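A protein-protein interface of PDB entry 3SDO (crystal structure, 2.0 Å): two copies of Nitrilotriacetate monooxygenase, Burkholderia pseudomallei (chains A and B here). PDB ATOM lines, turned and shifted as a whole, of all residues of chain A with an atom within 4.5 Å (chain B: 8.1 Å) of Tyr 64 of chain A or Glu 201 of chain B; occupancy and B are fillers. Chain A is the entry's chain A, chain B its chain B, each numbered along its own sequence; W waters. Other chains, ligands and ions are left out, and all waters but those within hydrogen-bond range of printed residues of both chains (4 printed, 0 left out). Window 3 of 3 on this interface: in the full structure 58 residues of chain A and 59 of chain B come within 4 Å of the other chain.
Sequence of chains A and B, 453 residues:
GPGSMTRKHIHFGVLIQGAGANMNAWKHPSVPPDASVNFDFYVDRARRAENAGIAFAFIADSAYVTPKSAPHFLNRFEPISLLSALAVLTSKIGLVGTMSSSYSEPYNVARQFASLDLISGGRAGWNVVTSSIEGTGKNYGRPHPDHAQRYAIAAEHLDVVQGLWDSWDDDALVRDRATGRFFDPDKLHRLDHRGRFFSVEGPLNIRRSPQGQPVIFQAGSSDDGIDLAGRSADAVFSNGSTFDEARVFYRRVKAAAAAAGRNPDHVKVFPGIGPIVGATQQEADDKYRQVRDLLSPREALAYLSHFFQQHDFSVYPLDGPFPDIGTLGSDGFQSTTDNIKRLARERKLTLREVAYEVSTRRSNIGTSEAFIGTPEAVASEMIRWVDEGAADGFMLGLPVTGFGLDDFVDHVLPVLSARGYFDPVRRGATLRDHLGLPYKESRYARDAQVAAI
O of Ala 63 of chain A lies within hydrogen-bond range of ND2 of Asn 139 of chain A (2.9 Å).
The side-chain hydroxyl of Tyr 107 of chain B is in hydrogen-bond range of the backbone NH of Asn 205 of chain B (3.5 Å).
The side-chain amide oxygen (OD1) of Asn 205 of chain B lies within hydrogen-bond range of the guanidinium group (NE) of Arg 111 of chain B (3.0 Å).
The side-chain carboxylate of Glu 201 of chain B is in salt-bridge range of the guanidinium group of Arg 190 of chain B (3.0 Å).
N of Asp 192 of chain B sits at hydrogen-bond distance from O of Glu 201 of chain B (2.9 Å).
The backbone carbonyl oxygen (O) of Val 200 of chain B sits at hydrogen-bond distance from the backbone NH (N) of His 193 of chain B.
The backbone carbonyl oxygen of Ser 62 of chain A lies within hydrogen-bond range of the guanidinium group of Arg 111 of chain B (3.4 Å).
The side-chain amide nitrogen (ND2) of Asn 205 of chain B is in hydrogen-bond range of the backbone carbonyl oxygen (O) of Ser 62 of chain A, at 2.9 Å.
The side-chain carboxylate of Glu 201 of chain B lies within hydrogen-bond range of the side-chain hydroxyl of Tyr 64 of chain A, 3.3 Å away.
The backbone carbonyl oxygen (O) of Lys 138 of chain A lies within hydrogen-bond range of the backbone NH (N) of Glu 201 of chain B (3.0 Å).
N of Gly 202 of chain B sits at hydrogen-bond distance from OD1 of Asn 139 of chain A.
Hydrophobic or aromatic side chains of chain B within 4 Å of the printed part of chain A: Tyr 107, Val 200 and Pro 203.
Of the 12 printed residues of chain A, 6 touch a printed residue of chain B.
Hydrophobic or aromatic side chains of chain A that line the printed part of chain B: Ala 63, Tyr 64 and Val 65.
Among the printed residues, no Asp or Glu carboxylate lies within 4 Å of a Lys or Arg side-chain nitrogen of the other chain.
Among the printed residues, pairs that only touch across the chains: Asn 139 of chain A with Tyr 107 of chain B, Val 65 of chain A with Asn 205 of chain B, Lys 138 of chain A with Val 200 of chain B, Val 65 of chain A with Pro 203 of chain B, Lys 138 of chain A with Ser 199 of chain B, Ala 63 of chain A with Tyr 107 of chain B, Asn 139 of chain A with Glu 201 of chain B, Asn 139 of chain A with Val 200 of chain B and Ala 63 of chain A with Asn 205 of chain B.
Water W1 lies within hydrogen-bond range of the side-chain hydroxyl of Ser 62 of chain A, the backbone carbonyl oxygen of Tyr 64 of chain A and the side-chain amide nitrogen of Asn 205 of chain B.
Water W3 lies within hydrogen-bond range of the backbone carbonyl oxygen (O) of Lys 138 of chain A (2.6 Å) and the side-chain hydroxyl (OG) of Ser 199 of chain B (2.9 Å).
Water W4 bridges O of Asn 139 of chain A (2.8 Å) and N of Tyr 107 of chain B (3.0 Å).
Water W2 lies within hydrogen-bond range of the backbone NH of Val 65 of chain A, the side-chain amide nitrogen of Asn 139 of chain A, the backbone carbonyl oxygen of Pro 203 of chain B and the backbone carbonyl oxygen of Gly 202 of chain B.
Of chain B, only Glu 201 comes within 4 Å of Tyr 64 of chain A.
Glu 201 of chain B touches just these residues of chain A: Tyr 64, Lys 138 and Asn 139.
Of the printed residues of chain A, Arg 111 of chain B touches Ser 62 (3.4 Å).
Of the printed residues of chain B, Lys 138 of chain A touches Ser 199, Val 200 and Glu 201.
Of the printed residues of chain A, Val 200 of chain B touches Lys 138 (3.5 Å) and Asn 139 (3.6 Å).
Printed residues of chain B within 4 Å of Ser 62 of chain A: Arg 111 and Asn 205.
Of the printed residues of chain A, Asn 205 of chain B touches Ser 62 (2.9 Å), Ala 63 (3.997 Å) and Val 65 (3.4 Å).
Ile 133 of chain A touches none of the printed residues of chain B.
Gly 163 of chain B touches none of the printed residues of chain A.
The nearest residue of chain B that does not touch Tyr 64 of chain A is Tyr 107 of chain B (4.2 Å).
The nearest printed residue of chain B that does not touch Lys 138 of chain A is Gly 202 of chain B (5.1 Å).
No position is printed for both chains.
Of the 14 pairs that touch across the chains among the printed residues, none has its exchanged pair printed and touching as well.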
ATOM      1  N   SER A  62      11.579  -1.909  -0.250  1.00  0.00           N
ATOM      2  CA  SER A  62      12.220  -3.042  -0.901  1.00  0.00           C
ATOM      3  C   SER A  62      13.632  -2.656  -1.309  1.00  0.00           C
ATOM      4  O   SER A  62      13.957  -1.471  -1.408  1.00  0.00           O
ATOM      5  CB  SER A  62      11.417  -3.472  -2.137  1.00  0.00           C
ATOM      6  OG  SER A  62      11.331  -2.406  -3.088  1.00  0.00           O
ATOM      7  N   ALA A  63      14.474  -3.661  -1.547  1.00  0.00           N
ATOM      8  CA  ALA A  63      15.850  -3.412  -1.971  1.00  0.00           C
ATOM      9  C   ALA A  63      16.299  -4.424  -3.021  1.00  0.00           C
ATOM     10  O   ALA A  63      17.435  -4.875  -2.997  1.00  0.00           O
ATOM     11  CB  ALA A  63      16.786  -3.428  -0.772  1.00  0.00           C
ATOM     12  N   TYR A  64      15.402  -4.742  -3.946  1.00  0.00           N
ATOM     13  CA  TYR A  64      15.653  -5.740  -4.992  1.00  0.00           C
ATOM     14  C   TYR A  64      14.735  -5.469  -6.163  1.00  0.00           C
ATOM     15  O   TYR A  64      13.539  -5.221  -5.977  1.00  0.00           O
ATOM     16  CB  TYR A  64      15.447  -7.169  -4.479  1.00  0.00           C
ATOM     17  CG  TYR A  64      15.866  -8.223  -5.478  1.00  0.00           C
ATOM     18  CD1 TYR A  64      17.205  -8.357  -5.845  1.00  0.00           C
ATOM     19  CD2 TYR A  64      14.933  -9.076  -6.068  1.00  0.00           C
ATOM     20  CE1 TYR A  64      17.605  -9.311  -6.762  1.00  0.00           C
ATOM     21  CE2 TYR A  64      15.335 -10.041  -7.002  1.00  0.00           C
ATOM     22  CZ  TYR A  64      16.676 -10.144  -7.337  1.00  0.00           C
ATOM     23  OH  TYR A  64      17.109 -11.074  -8.267  1.00  0.00           O
ATOM     24  N   VAL A  65      15.312  -5.519  -7.358  1.00  0.00           N
ATOM     25  CA  VAL A  65      14.618  -5.207  -8.602  1.00  0.00           C
ATOM     26  C   VAL A  65      14.950  -6.238  -9.636  1.00  0.00           C
ATOM     27  O   VAL A  65      16.098  -6.696  -9.697  1.00  0.00           O
ATOM     28  CB  VAL A  65      15.096  -3.848  -9.192  1.00  0.00           C
ATOM     29  CG1 VAL A  65      14.554  -3.622 -10.621  1.00  0.00           C
ATOM     30  CG2 VAL A  65      14.692  -2.756  -8.319  1.00  0.00           C
ATOM     31  N   THR A  66      13.941  -6.615 -10.427  1.00  0.00           N
ATOM     32  CA  THR A  66      14.142  -7.340 -11.690  1.00  0.00           C
ATOM     33  C   THR A  66      13.288  -6.669 -12.763  1.00  0.00           C
ATOM     34  O   THR A  66      12.393  -5.892 -12.447  1.00  0.00           O
ATOM     35  CB  THR A  66      13.711  -8.833 -11.618  1.00  0.00           C
ATOM     36  OG1 THR A  66      12.287  -8.925 -11.774  1.00  0.00           O
ATOM     37  CG2 THR A  66      14.132  -9.488 -10.313  1.00  0.00           C
ATOM     38  N   SER A  69       9.596  -6.581 -11.929  1.00  0.00           N
ATOM     39  CA  SER A  69       9.086  -5.950 -10.707  1.00  0.00           C
ATOM     40  C   SER A  69       7.940  -4.998 -11.037  1.00  0.00           C
ATOM     41  O   SER A  69       7.917  -4.397 -12.124  1.00  0.00           O
ATOM     42  CB  SER A  69      10.195  -5.159  -9.997  1.00  0.00           C
ATOM     43  OG  SER A  69      11.299  -5.981  -9.646  1.00  0.00           O
ATOM     44  N   ILE A 133      12.280  -9.677   0.199  1.00  0.00           N
ATOM     45  CA  ILE A 133      12.004 -10.288  -1.111  1.00  0.00           C
ATOM     46  C   ILE A 133      13.120 -11.258  -1.457  1.00  0.00           C
ATOM     47  O   ILE A 133      14.302 -10.935  -1.266  1.00  0.00           O
ATOM     48  CB  ILE A 133      12.015  -9.252  -2.281  1.00  0.00           C
ATOM     49  CG1 ILE A 133      10.851  -8.280  -2.212  1.00  0.00           C
ATOM     50  CG2 ILE A 133      11.963  -9.970  -3.643  1.00  0.00           C
ATOM     51  CD1 ILE A 133      10.919  -7.204  -3.308  1.00  0.00           C
ATOM     52  N   GLU A 134      12.759 -12.422  -1.991  1.00  0.00           N
ATOM     53  CA  GLU A 134      13.753 -13.392  -2.422  1.00  0.00           C
ATOM     54  C   GLU A 134      14.658 -12.747  -3.471  1.00  0.00           C
ATOM     55  O   GLU A 134      14.159 -12.166  -4.440  1.00  0.00           O
ATOM     56  CB  GLU A 134      13.100 -14.672  -2.996  1.00  0.00           C
ATOM     57  CG  GLU A 134      14.007 -15.909  -2.879  1.00  0.00           C
ATOM     58  CD  GLU A 134      13.673 -17.034  -3.843  1.00  0.00           C
ATOM     59  OE1 GLU A 134      12.708 -16.916  -4.639  1.00  0.00           O
ATOM     60  OE2 GLU A 134      14.394 -18.066  -3.794  1.00  0.00           O
ATOM     61  N   GLY A 135      15.974 -12.843  -3.259  1.00  0.00           N
ATOM     62  CA  GLY A 135      16.966 -12.213  -4.137  1.00  0.00           C
ATOM     63  C   GLY A 135      17.658 -10.980  -3.554  1.00  0.00           C
ATOM     64  O   GLY A 135      18.734 -10.598  -4.012  1.00  0.00           O
ATOM     65  N   THR A 136      17.043 -10.338  -2.558  1.00  0.00           N
ATOM     66  CA  THR A 136      17.603  -9.140  -1.936  1.00  0.00           C
ATOM     67  C   THR A 136      19.056  -9.300  -1.525  1.00  0.00           C
ATOM     68  O   THR A 136      19.853  -8.397  -1.719  1.00  0.00           O
ATOM     69  CB  THR A 136      16.775  -8.704  -0.703  1.00  0.00           C
ATOM     70  OG1 THR A 136      15.400  -8.574  -1.088  1.00  0.00           O
ATOM     71  CG2 THR A 136      17.282  -7.331  -0.127  1.00  0.00           C
ATOM     72  N   LYS A 138      21.390 -10.758  -2.853  1.00  0.00           N
ATOM     73  CA  LYS A 138      22.268 -10.544  -3.997  1.00  0.00           C
ATOM     74  C   LYS A 138      22.794  -9.101  -4.110  1.00  0.00           C
ATOM     75  O   LYS A 138      23.792  -8.868  -4.801  1.00  0.00           O
ATOM     76  CB  LYS A 138      21.557 -10.950  -5.315  1.00  0.00           C
ATOM     77  CG  LYS A 138      21.366 -12.443  -5.471  1.00  0.00           C
ATOM     78  CD  LYS A 138      20.366 -12.785  -6.581  1.00  0.00           C
ATOM     79  CE  LYS A 138      20.511 -14.235  -7.005  1.00  0.00           C
ATOM     80  NZ  LYS A 138      19.247 -14.804  -7.527  1.00  0.00           N
ATOM     81  N   ASN A 139      22.121  -8.150  -3.457  1.00  0.00           N
ATOM     82  CA  ASN A 139      22.597  -6.765  -3.412  1.00  0.00           C
ATOM     83  C   ASN A 139      23.498  -6.448  -2.224  1.00  0.00           C
ATOM     84  O   ASN A 139      23.916  -5.300  -2.062  1.00  0.00           O
ATOM     85  CB  ASN A 139      21.411  -5.791  -3.479  1.00  0.00           C
ATOM     86  CG  ASN A 139      20.786  -5.776  -4.841  1.00  0.00           C
ATOM     87  OD1 ASN A 139      21.473  -6.036  -5.823  1.00  0.00           O
ATOM     88  ND2 ASN A 139      19.489  -5.477  -4.922  1.00  0.00           N
ATOM     89  N   TYR B 107      24.939  -0.718  -1.571  1.00  0.00           N
ATOM     90  CA  TYR B 107      23.552  -0.610  -2.065  1.00  0.00           C
ATOM     91  C   TYR B 107      22.747   0.377  -1.220  1.00  0.00           C
ATOM     92  O   TYR B 107      21.969   1.177  -1.763  1.00  0.00           O
ATOM     93  CB  TYR B 107      22.877  -1.984  -2.137  1.00  0.00           C
ATOM     94  CG  TYR B 107      21.660  -2.026  -3.027  1.00  0.00           C
ATOM     95  CD1 TYR B 107      21.791  -2.272  -4.392  1.00  0.00           C
ATOM     96  CD2 TYR B 107      20.369  -1.847  -2.509  1.00  0.00           C
ATOM     97  CE1 TYR B 107      20.703  -2.320  -5.216  1.00  0.00           C
ATOM     98  CE2 TYR B 107      19.255  -1.892  -3.346  1.00  0.00           C
ATOM     99  CZ  TYR B 107      19.436  -2.146  -4.706  1.00  0.00           C
ATOM    100  OH  TYR B 107      18.362  -2.206  -5.579  1.00  0.00           O
ATOM    101  N   ARG B 111      21.343   4.096  -2.459  1.00  0.00           N
ATOM    102  CA  ARG B 111      19.922   4.447  -2.337  1.00  0.00           C
ATOM    103  C   ARG B 111      19.718   5.720  -1.522  1.00  0.00           C
ATOM    104  O   ARG B 111      18.982   6.615  -1.917  1.00  0.00           O
ATOM    105  CB  ARG B 111      19.133   3.318  -1.674  1.00  0.00           C
ATOM    106  CG  ARG B 111      18.881   2.103  -2.519  1.00  0.00           C
ATOM    107  CD  ARG B 111      17.963   1.186  -1.735  1.00  0.00           C
ATOM    108  NE  ARG B 111      16.591   1.674  -1.768  1.00  0.00           N
ATOM    109  CZ  ARG B 111      15.661   1.424  -0.856  1.00  0.00           C
ATOM    110  NH1 ARG B 111      15.935   0.735   0.267  1.00  0.00           N
ATOM    111  NH2 ARG B 111      14.434   1.877  -1.073  1.00  0.00           N
ATOM    112  N   VAL B 160      31.155   0.525  -6.970  1.00  0.00           N
ATOM    113  CA  VAL B 160      29.852  -0.115  -6.899  1.00  0.00           C
ATOM    114  C   VAL B 160      28.740   0.930  -6.838  1.00  0.00           C
ATOM    115  O   VAL B 160      27.741   0.810  -7.524  1.00  0.00           O
ATOM    116  CB  VAL B 160      29.738  -1.049  -5.686  1.00  0.00           C
ATOM    117  CG1 VAL B 160      28.287  -1.564  -5.542  1.00  0.00           C
ATOM    118  CG2 VAL B 160      30.739  -2.238  -5.823  1.00  0.00           C
ATOM    119  N   GLY B 163      28.312   2.705 -10.191  1.00  0.00           N
ATOM    120  CA  GLY B 163      27.683   1.761 -11.135  1.00  0.00           C
ATOM    121  C   GLY B 163      26.185   1.624 -10.863  1.00  0.00           C
ATOM    122  O   GLY B 163      25.355   1.594 -11.786  1.00  0.00           O
ATOM    123  N   LEU B 164      25.835   1.557  -9.580  1.00  0.00           N
ATOM    124  CA  LEU B 164      24.451   1.429  -9.193  1.00  0.00           C
ATOM    125  C   LEU B 164      23.656   2.678  -9.599  1.00  0.00           C
ATOM    126  O   LEU B 164      22.532   2.588 -10.089  1.00  0.00           O
ATOM    127  CB  LEU B 164      24.328   1.160  -7.681  1.00  0.00           C
ATOM    128  CG  LEU B 164      24.689  -0.209  -7.126  1.00  0.00           C
ATOM    129  CD1 LEU B 164      24.618  -0.121  -5.602  1.00  0.00           C
ATOM    130  CD2 LEU B 164      23.741  -1.321  -7.690  1.00  0.00           C
ATOM    131  N   SER B 167      22.006   2.725 -12.970  1.00  0.00           N
ATOM    132  CA  SER B 167      21.045   1.648 -13.254  1.00  0.00           C
ATOM    133  C   SER B 167      19.982   2.089 -14.249  1.00  0.00           C
ATOM    134  O   SER B 167      19.650   1.339 -15.181  1.00  0.00           O
ATOM    135  CB  SER B 167      20.357   1.155 -11.984  1.00  0.00           C
ATOM    136  OG  SER B 167      21.268   0.523 -11.111  1.00  0.00           O
ATOM    137  N   HIS B 189      19.785  -1.248 -16.351  1.00  0.00           N
ATOM    138  CA  HIS B 189      20.993  -2.075 -16.401  1.00  0.00           C
ATOM    139  C   HIS B 189      21.275  -2.756 -15.055  1.00  0.00           C
ATOM    140  O   HIS B 189      21.129  -2.145 -13.995  1.00  0.00           O
ATOM    141  CB  HIS B 189      22.220  -1.228 -16.767  1.00  0.00           C
ATOM    142  CG  HIS B 189      22.021  -0.344 -17.960  1.00  0.00           C
ATOM    143  ND1 HIS B 189      22.515  -0.662 -19.210  1.00  0.00           N
ATOM    144  CD2 HIS B 189      21.384   0.844 -18.092  1.00  0.00           C
ATOM    145  CE1 HIS B 189      22.176   0.291 -20.064  1.00  0.00           C
ATOM    146  NE2 HIS B 189      21.493   1.221 -19.409  1.00  0.00           N
ATOM    147  N   ARG B 190      21.694  -4.016 -15.109  1.00  0.00           N
ATOM    148  CA  ARG B 190      22.253  -4.694 -13.941  1.00  0.00           C
ATOM    149  C   ARG B 190      23.696  -4.267 -13.778  1.00  0.00           C
ATOM    150  O   ARG B 190      24.318  -3.775 -14.728  1.00  0.00           O
ATOM    151  CB  ARG B 190      22.217  -6.207 -14.112  1.00  0.00           C
ATOM    152  CG  ARG B 190      20.826  -6.775 -14.211  1.00  0.00           C
ATOM    153  CD  ARG B 190      20.875  -8.242 -14.578  1.00  0.00           C
ATOM    154  NE  ARG B 190      21.169  -9.093 -13.426  1.00  0.00           N
ATOM    155  CZ  ARG B 190      22.136 -10.007 -13.377  1.00  0.00           C
ATOM    156  NH1 ARG B 190      22.934 -10.233 -14.416  1.00  0.00           N
ATOM    157  NH2 ARG B 190      22.300 -10.741 -12.285  1.00  0.00           N
ATOM    158  N   LEU B 191      24.233  -4.448 -12.579  1.00  0.00           N
ATOM    159  CA  LEU B 191      25.650  -4.144 -12.321  1.00  0.00           C
ATOM    160  C   LEU B 191      26.471  -5.430 -12.390  1.00  0.00           C
ATOM    161  O   LEU B 191      27.501  -5.480 -13.059  1.00  0.00           O
ATOM    162  CB  LEU B 191      25.808  -3.462 -10.945  1.00  0.00           C
ATOM    163  CG  LEU B 191      27.196  -2.947 -10.542  1.00  0.00           C
ATOM    164  CD1 LEU B 191      27.677  -1.876 -11.511  1.00  0.00           C
ATOM    165  CD2 LEU B 191      27.197  -2.422  -9.108  1.00  0.00           C
ATOM    166  N   ASP B 192      26.002  -6.467 -11.697  1.00  0.00           N
ATOM    167  CA  ASP B 192      26.718  -7.743 -11.565  1.00  0.00           C
ATOM    168  C   ASP B 192      28.158  -7.529 -11.170  1.00  0.00           C
ATOM    169  O   ASP B 192      29.065  -7.985 -11.865  1.00  0.00           O
ATOM    170  CB  ASP B 192      26.705  -8.540 -12.874  1.00  0.00           C
ATOM    171  CG  ASP B 192      25.357  -9.071 -13.208  1.00  0.00           C
ATOM    172  OD1 ASP B 192      24.916 -10.030 -12.555  1.00  0.00           O
ATOM    173  OD2 ASP B 192      24.735  -8.523 -14.144  1.00  0.00           O
ATOM    174  N   HIS B 193      28.363  -6.799 -10.084  1.00  0.00           N
ATOM    175  CA  HIS B 193      29.698  -6.576  -9.563  1.00  0.00           C
ATOM    176  C   HIS B 193      30.084  -7.748  -8.670  1.00  0.00           C
ATOM    177  O   HIS B 193      29.373  -8.057  -7.712  1.00  0.00           O
ATOM    178  CB  HIS B 193      29.724  -5.294  -8.738  1.00  0.00           C
ATOM    179  CG  HIS B 193      31.037  -5.028  -8.082  1.00  0.00           C
ATOM    180  ND1 HIS B 193      31.994  -4.219  -8.648  1.00  0.00           N
ATOM    181  CD2 HIS B 193      31.544  -5.450  -6.900  1.00  0.00           C
ATOM    182  CE1 HIS B 193      33.041  -4.157  -7.845  1.00  0.00           C
ATOM    183  NE2 HIS B 193      32.790  -4.888  -6.773  1.00  0.00           N
ATOM    184  N   ARG B 194      31.194  -8.398  -9.002  1.00  0.00           N
ATOM    185  CA  ARG B 194      31.820  -9.396  -8.149  1.00  0.00           C
ATOM    186  C   ARG B 194      33.294  -8.986  -8.034  1.00  0.00           C
ATOM    187  O   ARG B 194      34.052  -9.137  -8.987  1.00  0.00           O
ATOM    188  CB  ARG B 194      31.670 -10.798  -8.767  1.00  0.00           C
ATOM    189  CG  ARG B 194      30.202 -11.139  -9.129  1.00  0.00           C
ATOM    190  CD  ARG B 194      30.009 -12.480  -9.872  1.00  0.00           C
ATOM    191  NE  ARG B 194      30.804 -12.588 -11.106  1.00  0.00           N
ATOM    192  CZ  ARG B 194      30.459 -12.117 -12.310  1.00  0.00           C
ATOM    193  NH1 ARG B 194      29.309 -11.477 -12.514  1.00  0.00           N
ATOM    194  NH2 ARG B 194      31.286 -12.297 -13.338  1.00  0.00           N
ATOM    195  N   PHE B 198      33.245  -6.731  -2.358  1.00  0.00           N
ATOM    196  CA  PHE B 198      31.806  -6.593  -2.528  1.00  0.00           C
ATOM    197  C   PHE B 198      31.253  -7.474  -3.648  1.00  0.00           C
ATOM    198  O   PHE B 198      31.914  -7.722  -4.663  1.00  0.00           O
ATOM    199  CB  PHE B 198      31.431  -5.116  -2.799  1.00  0.00           C
ATOM    200  CG  PHE B 198      31.880  -4.175  -1.716  1.00  0.00           C
ATOM    201  CD1 PHE B 198      31.210  -4.133  -0.496  1.00  0.00           C
ATOM    202  CD2 PHE B 198      33.012  -3.367  -1.889  1.00  0.00           C
ATOM    203  CE1 PHE B 198      31.653  -3.291   0.538  1.00  0.00           C
ATOM    204  CE2 PHE B 198      33.442  -2.522  -0.867  1.00  0.00           C
ATOM    205  CZ  PHE B 198      32.761  -2.484   0.341  1.00  0.00           C
ATOM    206  N   SER B 199      30.025  -7.926  -3.440  1.00  0.00           N
ATOM    207  CA  SER B 199      29.256  -8.603  -4.478  1.00  0.00           C
ATOM    208  C   SER B 199      27.824  -8.084  -4.511  1.00  0.00           C
ATOM    209  O   SER B 199      27.035  -8.314  -3.588  1.00  0.00           O
ATOM    210  CB  SER B 199      29.300 -10.122  -4.291  1.00  0.00           C
ATOM    211  OG  SER B 199      28.704 -10.716  -5.411  1.00  0.00           O
ATOM    212  N   VAL B 200      27.509  -7.347  -5.575  1.00  0.00           N
ATOM    213  CA  VAL B 200      26.258  -6.596  -5.665  1.00  0.00           C
ATOM    214  C   VAL B 200      25.736  -6.657  -7.097  1.00  0.00           C
ATOM    215  O   VAL B 200      26.382  -6.174  -8.044  1.00  0.00           O
ATOM    216  CB  VAL B 200      26.470  -5.122  -5.236  1.00  0.00           C
ATOM    217  CG1 VAL B 200      25.156  -4.310  -5.342  1.00  0.00           C
ATOM    218  CG2 VAL B 200      27.081  -5.057  -3.810  1.00  0.00           C
ATOM    219  N   GLU B 201      24.562  -7.252  -7.242  1.00  0.00           N
ATOM    220  CA  GLU B 201      23.969  -7.507  -8.550  1.00  0.00           C
ATOM    221  C   GLU B 201      23.312  -6.298  -9.215  1.00  0.00           C
ATOM    222  O   GLU B 201      23.449  -6.092 -10.426  1.00  0.00           O
ATOM    223  CB  GLU B 201      22.957  -8.628  -8.398  1.00  0.00           C
ATOM    224  CG  GLU B 201      22.145  -8.892  -9.625  1.00  0.00           C
ATOM    225  CD  GLU B 201      21.229 -10.091  -9.457  1.00  0.00           C
ATOM    226  OE1 GLU B 201      21.757 -11.219  -9.377  1.00  0.00           O
ATOM    227  OE2 GLU B 201      19.997  -9.891  -9.439  1.00  0.00           O
ATOM    228  N   GLY B 202      22.608  -5.480  -8.438  1.00  0.00           N
ATOM    229  CA  GLY B 202      21.775  -4.443  -9.020  1.00  0.00           C
ATOM    230  C   GLY B 202      20.560  -5.082  -9.707  1.00  0.00           C
ATOM    231  O   GLY B 202      20.372  -6.285  -9.658  1.00  0.00           O
ATOM    232  N   PRO B 203      19.720  -4.279 -10.343  1.00  0.00           N
ATOM    233  CA  PRO B 203      19.820  -2.817 -10.435  1.00  0.00           C
ATOM    234  C   PRO B 203      19.413  -2.103  -9.142  1.00  0.00           C
ATOM    235  O   PRO B 203      18.794  -2.708  -8.256  1.00  0.00           O
ATOM    236  CB  PRO B 203      18.819  -2.471 -11.543  1.00  0.00           C
ATOM    237  CG  PRO B 203      18.484  -3.817 -12.222  1.00  0.00           C
ATOM    238  CD  PRO B 203      18.620  -4.824 -11.158  1.00  0.00           C
ATOM    239  N   LEU B 204      19.752  -0.824  -9.056  1.00  0.00           N
ATOM    240  CA  LEU B 204      19.221   0.065  -8.016  1.00  0.00           C
ATOM    241  C   LEU B 204      17.744   0.318  -8.302  1.00  0.00           C
ATOM    242  O   LEU B 204      17.322   0.311  -9.462  1.00  0.00           O
ATOM    243  CB  LEU B 204      19.990   1.404  -8.024  1.00  0.00           C
ATOM    244  CG  LEU B 204      19.889   2.317  -6.794  1.00  0.00           C
ATOM    245  CD1 LEU B 204      20.386   1.568  -5.541  1.00  0.00           C
ATOM    246  CD2 LEU B 204      20.659   3.631  -6.975  1.00  0.00           C
ATOM    247  N   ASN B 205      16.962   0.529  -7.246  1.00  0.00           N
ATOM    248  CA  ASN B 205      15.538   0.841  -7.373  1.00  0.00           C
ATOM    249  C   ASN B 205      15.208   2.329  -7.204  1.00  0.00           C
ATOM    250  O   ASN B 205      14.175   2.702  -6.641  1.00  0.00           O
ATOM    251  CB  ASN B 205      14.729  -0.003  -6.410  1.00  0.00           C
ATOM    252  CG  ASN B 205      15.055   0.269  -4.980  1.00  0.00           C
ATOM    253  OD1 ASN B 205      15.952   1.058  -4.666  1.00  0.00           O
ATOM    254  ND2 ASN B 205      14.325  -0.383  -4.086  1.00  0.00           N
HETATM  255  O   HOH W   1      12.613  -2.537  -5.298  1.00  0.00           O
HETATM  256  O   HOH W   2      18.183  -5.540  -7.507  1.00  0.00           O
HETATM  257  O   HOH W   3      25.821 -10.471  -5.366  1.00  0.00           O
HETATM  258  O   HOH W   4      25.567  -3.496  -0.731  1.00  0.00           O
